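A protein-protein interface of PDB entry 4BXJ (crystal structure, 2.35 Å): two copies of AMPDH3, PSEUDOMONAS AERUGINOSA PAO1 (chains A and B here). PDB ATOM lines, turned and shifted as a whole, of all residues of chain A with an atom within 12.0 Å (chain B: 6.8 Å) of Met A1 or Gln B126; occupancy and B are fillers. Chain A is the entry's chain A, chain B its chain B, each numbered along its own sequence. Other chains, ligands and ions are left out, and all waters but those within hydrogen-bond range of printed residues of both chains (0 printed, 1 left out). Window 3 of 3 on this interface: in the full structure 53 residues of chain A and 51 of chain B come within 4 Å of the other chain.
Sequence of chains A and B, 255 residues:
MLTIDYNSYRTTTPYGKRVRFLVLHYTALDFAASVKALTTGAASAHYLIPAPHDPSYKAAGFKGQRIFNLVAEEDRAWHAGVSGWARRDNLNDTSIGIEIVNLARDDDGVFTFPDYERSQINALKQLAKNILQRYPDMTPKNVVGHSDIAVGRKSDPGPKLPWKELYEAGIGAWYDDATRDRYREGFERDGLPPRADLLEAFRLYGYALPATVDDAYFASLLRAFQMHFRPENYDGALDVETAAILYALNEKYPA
Printed residues of chain A that touch a printed residue of chain B: Met A1, Leu A2, Ile A4 and Asp A5. Of the 14 printed residues of chain B, 4 touch a printed residue of chain A.
Met A1 touches just one residue of chain B: Gln B126 (3.8 Å). Of the printed residues of chain B, Leu A2 touches Ile B67 (3.6 Å), Ala B123 (3.7 Å) and Gln B126 (2.8 Å). Of the printed residues of chain B, Ile A4 touches Ile B67 and Leu B127. Of the printed residues of chain B, Asp A5 touches Ile B67. Printed residues of chain A within 4 Å of Ile B67: Leu A2, Ile A4 and Asp A5. Asn B122 touches none of the printed residues of chain A. Of chain A, only Leu A2 (3.7 Å) comes within 4 Å of Ala B123. No residue of chain A comes within 4 Å of Lys B125. Of the printed residues of chain A, Leu B127 touches Ile A4 (3.8 Å). No residue of chain A comes within 4 Å of Ala B128. No residue of chain A comes within 4 Å of Lys B129. No residue of chain A comes within 4 Å of Asn B130. Ile B171 touches none of the printed residues of chain A. The nearest printed residue of chain B that does not touch Leu A2 is Asn B122 (5.9 Å).
Among the printed residues, pairs that only touch across the chains: Leu A2 with Ile B67 (3.6 Å), Ile A4 with Ile B67 (3.7 Å), Leu A2 with Ala B123 (3.7 Å), Ile A4 with Leu B127 (3.8 Å) and Met A1 with Gln B126 (3.8 Å).
O of Leu A2 sits at hydrogen-bond distance from NE2 of Gln B126 (2.8 Å). N of Asp A5 sits at hydrogen-bond distance from O of Ile B67 (2.8 Å).
No position is printed for both chains. Of the 7 pairs that touch across the chains among the printed residues, none has its exchanged pair printed and touching as well.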
ATOM      1  N   MET A   1     -13.001 -18.649  -7.420  1.00  0.00           N
ATOM      2  CA  MET A   1     -13.555 -17.387  -7.910  1.00  0.00           C
ATOM      3  C   MET A   1     -14.796 -17.619  -8.778  1.00  0.00           C
ATOM      4  O   MET A   1     -14.795 -17.424 -10.005  1.00  0.00           O
ATOM      5  CB  MET A   1     -12.497 -16.559  -8.649  1.00  0.00           C
ATOM      6  CG  MET A   1     -12.968 -15.151  -9.056  1.00  0.00           C
ATOM      7  SD  MET A   1     -13.412 -14.025  -7.702  1.00  0.00           S
ATOM      8  CE  MET A   1     -12.865 -12.497  -8.435  1.00  0.00           C
ATOM      9  N   LEU A   2     -15.857 -18.046  -8.107  1.00  0.00           N
ATOM     10  CA  LEU A   2     -17.159 -18.180  -8.720  1.00  0.00           C
ATOM     11  C   LEU A   2     -17.749 -16.802  -8.911  1.00  0.00           C
ATOM     12  O   LEU A   2     -17.454 -15.875  -8.153  1.00  0.00           O
ATOM     13  CB  LEU A   2     -18.088 -18.971  -7.811  1.00  0.00           C
ATOM     14  CG  LEU A   2     -17.619 -20.346  -7.346  1.00  0.00           C
ATOM     15  CD1 LEU A   2     -18.750 -21.080  -6.650  1.00  0.00           C
ATOM     16  CD2 LEU A   2     -17.101 -21.144  -8.535  1.00  0.00           C
ATOM     17  N   THR A   3     -18.581 -16.668  -9.933  1.00  0.00           N
ATOM     18  CA  THR A   3     -19.428 -15.499 -10.076  1.00  0.00           C
ATOM     19  C   THR A   3     -20.832 -15.987  -9.774  1.00  0.00           C
ATOM     20  O   THR A   3     -21.141 -17.153  -9.993  1.00  0.00           O
ATOM     21  CB  THR A   3     -19.328 -14.918 -11.491  1.00  0.00           C
ATOM     22  OG1 THR A   3     -17.947 -14.720 -11.822  1.00  0.00           O
ATOM     23  CG2 THR A   3     -20.041 -13.584 -11.576  1.00  0.00           C
ATOM     24  N   ILE A   4     -21.678 -15.123  -9.229  1.00  0.00           N
ATOM     25  CA  ILE A   4     -23.053 -15.531  -8.921  1.00  0.00           C
ATOM     26  C   ILE A   4     -23.919 -15.597 -10.198  1.00  0.00           C
ATOM     27  O   ILE A   4     -23.735 -14.800 -11.124  1.00  0.00           O
ATOM     28  CB  ILE A   4     -23.658 -14.637  -7.826  1.00  0.00           C
ATOM     29  CG1 ILE A   4     -22.691 -14.578  -6.643  1.00  0.00           C
ATOM     30  CG2 ILE A   4     -25.026 -15.143  -7.395  1.00  0.00           C
ATOM     31  CD1 ILE A   4     -23.287 -14.108  -5.356  1.00  0.00           C
ATOM     32  N   ASP A   5     -24.812 -16.591 -10.260  1.00  0.00           N
ATOM     33  CA  ASP A   5     -25.679 -16.807 -11.423  1.00  0.00           C
ATOM     34  C   ASP A   5     -27.042 -16.190 -11.147  1.00  0.00           C
ATOM     35  O   ASP A   5     -27.826 -16.724 -10.354  1.00  0.00           O
ATOM     36  CB  ASP A   5     -25.836 -18.309 -11.694  1.00  0.00           C
ATOM     37  CG  ASP A   5     -26.543 -18.621 -13.033  1.00  0.00           C
ATOM     38  OD1 ASP A   5     -27.204 -17.738 -13.652  1.00  0.00           O
ATOM     39  OD2 ASP A   5     -26.435 -19.793 -13.459  1.00  0.00           O
ATOM     40  N   TYR A   6     -27.319 -15.064 -11.795  1.00  0.00           N
ATOM     41  CA  TYR A   6     -28.580 -14.366 -11.589  1.00  0.00           C
ATOM     42  C   TYR A   6     -29.539 -14.616 -12.744  1.00  0.00           C
ATOM     43  O   TYR A   6     -30.600 -13.998 -12.821  1.00  0.00           O
ATOM     44  CB  TYR A   6     -28.338 -12.862 -11.504  1.00  0.00           C
ATOM     45  CG  TYR A   6     -27.420 -12.411 -10.404  1.00  0.00           C
ATOM     46  CD1 TYR A   6     -27.900 -12.192  -9.118  1.00  0.00           C
ATOM     47  CD2 TYR A   6     -26.079 -12.174 -10.649  1.00  0.00           C
ATOM     48  CE1 TYR A   6     -27.070 -11.761  -8.104  1.00  0.00           C
ATOM     49  CE2 TYR A   6     -25.233 -11.738  -9.630  1.00  0.00           C
ATOM     50  CZ  TYR A   6     -25.738 -11.532  -8.363  1.00  0.00           C
ATOM     51  OH  TYR A   6     -24.905 -11.099  -7.357  1.00  0.00           O
ATOM     52  N   ILE B  67     -22.946 -20.835  -7.949  1.00  0.00           N
ATOM     53  CA  ILE B  67     -23.885 -20.307  -6.956  1.00  0.00           C
ATOM     54  C   ILE B  67     -25.067 -19.626  -7.644  1.00  0.00           C
ATOM     55  O   ILE B  67     -24.890 -18.723  -8.477  1.00  0.00           O
ATOM     56  CB  ILE B  67     -23.221 -19.285  -6.019  1.00  0.00           C
ATOM     57  CG1 ILE B  67     -22.026 -19.916  -5.297  1.00  0.00           C
ATOM     58  CG2 ILE B  67     -24.234 -18.766  -5.011  1.00  0.00           C
ATOM     59  CD1 ILE B  67     -21.007 -18.917  -4.791  1.00  0.00           C
ATOM     60  N   ILE B 121     -18.521 -26.343  -0.132  1.00  0.00           N
ATOM     61  CA  ILE B 121     -18.090 -25.634   1.059  1.00  0.00           C
ATOM     62  C   ILE B 121     -17.202 -24.458   0.684  1.00  0.00           C
ATOM     63  O   ILE B 121     -17.233 -23.415   1.329  1.00  0.00           O
ATOM     64  CB  ILE B 121     -17.382 -26.588   2.039  1.00  0.00           C
ATOM     65  CG1 ILE B 121     -18.364 -27.652   2.512  1.00  0.00           C
ATOM     66  CG2 ILE B 121     -16.828 -25.845   3.233  1.00  0.00           C
ATOM     67  CD1 ILE B 121     -19.487 -27.110   3.337  1.00  0.00           C
ATOM     68  N   ASN B 122     -16.406 -24.606  -0.362  1.00  0.00           N
ATOM     69  CA  ASN B 122     -15.588 -23.480  -0.783  1.00  0.00           C
ATOM     70  C   ASN B 122     -16.452 -22.382  -1.369  1.00  0.00           C
ATOM     71  O   ASN B 122     -16.116 -21.207  -1.277  1.00  0.00           O
ATOM     72  CB  ASN B 122     -14.523 -23.904  -1.784  1.00  0.00           C
ATOM     73  CG  ASN B 122     -13.487 -24.816  -1.171  1.00  0.00           C
ATOM     74  OD1 ASN B 122     -13.212 -24.757   0.034  1.00  0.00           O
ATOM     75  ND2 ASN B 122     -12.906 -25.675  -1.996  1.00  0.00           N
ATOM     76  N   ALA B 123     -17.574 -22.782  -1.961  1.00  0.00           N
ATOM     77  CA  ALA B 123     -18.528 -21.844  -2.517  1.00  0.00           C
ATOM     78  C   ALA B 123     -19.171 -21.099  -1.367  1.00  0.00           C
ATOM     79  O   ALA B 123     -19.290 -19.873  -1.395  1.00  0.00           O
ATOM     80  CB  ALA B 123     -19.577 -22.570  -3.316  1.00  0.00           C
ATOM     81  N   LEU B 124     -19.555 -21.849  -0.342  1.00  0.00           N
ATOM     82  CA  LEU B 124     -20.286 -21.288   0.785  1.00  0.00           C
ATOM     83  C   LEU B 124     -19.446 -20.292   1.551  1.00  0.00           C
ATOM     84  O   LEU B 124     -19.954 -19.309   2.062  1.00  0.00           O
ATOM     85  CB  LEU B 124     -20.764 -22.396   1.717  1.00  0.00           C
ATOM     86  CG  LEU B 124     -21.415 -21.965   3.028  1.00  0.00           C
ATOM     87  CD1 LEU B 124     -22.643 -21.084   2.792  1.00  0.00           C
ATOM     88  CD2 LEU B 124     -21.766 -23.198   3.849  1.00  0.00           C
ATOM     89  N   LYS B 125     -18.151 -20.545   1.634  1.00  0.00           N
ATOM     90  CA  LYS B 125     -17.267 -19.633   2.323  1.00  0.00           C
ATOM     91  C   LYS B 125     -17.109 -18.351   1.518  1.00  0.00           C
ATOM     92  O   LYS B 125     -17.109 -17.253   2.070  1.00  0.00           O
ATOM     93  CB  LYS B 125     -15.914 -20.292   2.563  1.00  0.00           C
ATOM     94  CG  LYS B 125     -15.848 -21.050   3.866  1.00  0.00           C
ATOM     95  CD  LYS B 125     -14.914 -22.255   3.791  1.00  0.00           C
ATOM     96  CE  LYS B 125     -13.507 -21.876   3.377  1.00  0.00           C
ATOM     97  NZ  LYS B 125     -12.606 -23.053   3.524  1.00  0.00           N
ATOM     98  N   GLN B 126     -16.967 -18.496   0.207  1.00  0.00           N
ATOM     99  CA  GLN B 126     -16.829 -17.344  -0.662  1.00  0.00           C
ATOM    100  C   GLN B 126     -18.100 -16.497  -0.591  1.00  0.00           C
ATOM    101  O   GLN B 126     -18.037 -15.279  -0.406  1.00  0.00           O
ATOM    102  CB  GLN B 126     -16.582 -17.793  -2.091  1.00  0.00           C
ATOM    103  CG  GLN B 126     -16.512 -16.654  -3.073  1.00  0.00           C
ATOM    104  CD  GLN B 126     -16.461 -17.138  -4.506  1.00  0.00           C
ATOM    105  OE1 GLN B 126     -15.770 -18.113  -4.820  1.00  0.00           O
ATOM    106  NE2 GLN B 126     -17.202 -16.466  -5.387  1.00  0.00           N
ATOM    107  N   LEU B 127     -19.250 -17.159  -0.711  1.00  0.00           N
ATOM    108  CA  LEU B 127     -20.545 -16.490  -0.702  1.00  0.00           C
ATOM    109  C   LEU B 127     -20.821 -15.710   0.579  1.00  0.00           C
ATOM    110  O   LEU B 127     -21.214 -14.534   0.528  1.00  0.00           O
ATOM    111  CB  LEU B 127     -21.674 -17.496  -0.931  1.00  0.00           C
ATOM    112  CG  LEU B 127     -23.072 -16.886  -0.886  1.00  0.00           C
ATOM    113  CD1 LEU B 127     -23.190 -15.787  -1.923  1.00  0.00           C
ATOM    114  CD2 LEU B 127     -24.138 -17.941  -1.107  1.00  0.00           C
ATOM    115  N   ALA B 128     -20.629 -16.368   1.720  1.00  0.00           N
ATOM    116  CA  ALA B 128     -21.006 -15.786   3.003  1.00  0.00           C
ATOM    117  C   ALA B 128     -20.046 -14.660   3.381  1.00  0.00           C
ATOM    118  O   ALA B 128     -20.417 -13.691   4.031  1.00  0.00           O
ATOM    119  CB  ALA B 128     -21.043 -16.862   4.079  1.00  0.00           C
ATOM    120  N   LYS B 129     -18.803 -14.802   2.960  1.00  0.00           N
ATOM    121  CA  LYS B 129     -17.828 -13.758   3.137  1.00  0.00           C
ATOM    122  C   LYS B 129     -18.255 -12.533   2.313  1.00  0.00           C
ATOM    123  O   LYS B 129     -18.151 -11.394   2.772  1.00  0.00           O
ATOM    124  CB  LYS B 129     -16.464 -14.279   2.684  1.00  0.00           C
ATOM    125  CG  LYS B 129     -15.262 -13.468   3.127  1.00  0.00           C
ATOM    126  CD  LYS B 129     -13.990 -14.093   2.576  1.00  0.00           C
ATOM    127  CE  LYS B 129     -13.632 -15.327   3.349  1.00  0.00           C
ATOM    128  NZ  LYS B 129     -12.835 -14.918   4.534  1.00  0.00           N
ATOM    129  N   ASN B 130     -18.750 -12.772   1.101  1.00  0.00           N
ATOM    130  CA  ASN B 130     -19.231 -11.687   0.255  1.00  0.00           C
ATOM    131  C   ASN B 130     -20.364 -10.914   0.933  1.00  0.00           C
ATOM    132  O   ASN B 130     -20.371  -9.688   0.973  1.00  0.00           O
ATOM    133  CB  ASN B 130     -19.699 -12.213  -1.103  1.00  0.00           C
ATOM    134  CG  ASN B 130     -19.917 -11.096  -2.105  1.00  0.00           C
ATOM    135  OD1 ASN B 130     -20.907 -10.378  -2.039  1.00  0.00           O
ATOM    136  ND2 ASN B 130     -18.973 -10.922  -3.020  1.00  0.00           N
ATOM    137  N   ILE B 131     -21.316 -11.660   1.469  1.00  0.00           N
ATOM    138  CA  ILE B 131     -22.446 -11.105   2.193  1.00  0.00           C
ATOM    139  C   ILE B 131     -22.070 -10.356   3.471  1.00  0.00           C
ATOM    140  O   ILE B 131     -22.551  -9.252   3.694  1.00  0.00           O
ATOM    141  CB  ILE B 131     -23.455 -12.209   2.511  1.00  0.00           C
ATOM    142  CG1 ILE B 131     -24.015 -12.782   1.213  1.00  0.00           C
ATOM    143  CG2 ILE B 131     -24.547 -11.714   3.448  1.00  0.00           C
ATOM    144  CD1 ILE B 131     -24.771 -14.063   1.411  1.00  0.00           C
ATOM    145  N   GLN B 133     -19.481  -8.807   4.479  1.00  0.00           N
ATOM    146  CA  GLN B 133     -18.746  -7.561   4.312  1.00  0.00           C
ATOM    147  C   GLN B 133     -19.679  -6.435   3.949  1.00  0.00           C
ATOM    148  O   GLN B 133     -19.295  -5.263   3.993  1.00  0.00           O
ATOM    149  CB  GLN B 133     -17.694  -7.693   3.213  1.00  0.00           C
ATOM    150  CG  GLN B 133     -16.647  -8.764   3.463  1.00  0.00           C
ATOM    151  CD  GLN B 133     -15.748  -8.974   2.258  1.00  0.00           C
ATOM    152  OE1 GLN B 133     -15.012  -9.961   2.186  1.00  0.00           O
ATOM    153  NE2 GLN B 133     -15.797  -8.042   1.307  1.00  0.00           N
ATOM    154  N   ILE B 171     -16.301 -16.352   9.060  1.00  0.00           N
ATOM    155  CA  ILE B 171     -17.737 -16.474   8.860  1.00  0.00           C
ATOM    156  C   ILE B 171     -18.369 -17.178  10.041  1.00  0.00           C
ATOM    157  O   ILE B 171     -18.270 -18.390  10.145  1.00  0.00           O
ATOM    158  CB  ILE B 171     -18.021 -17.310   7.599  1.00  0.00           C
ATOM    159  CG1 ILE B 171     -17.427 -16.621   6.379  1.00  0.00           C
ATOM    160  CG2 ILE B 171     -19.515 -17.574   7.414  1.00  0.00           C
ATOM    161  CD1 ILE B 171     -17.375 -17.499   5.183  1.00  0.00           C
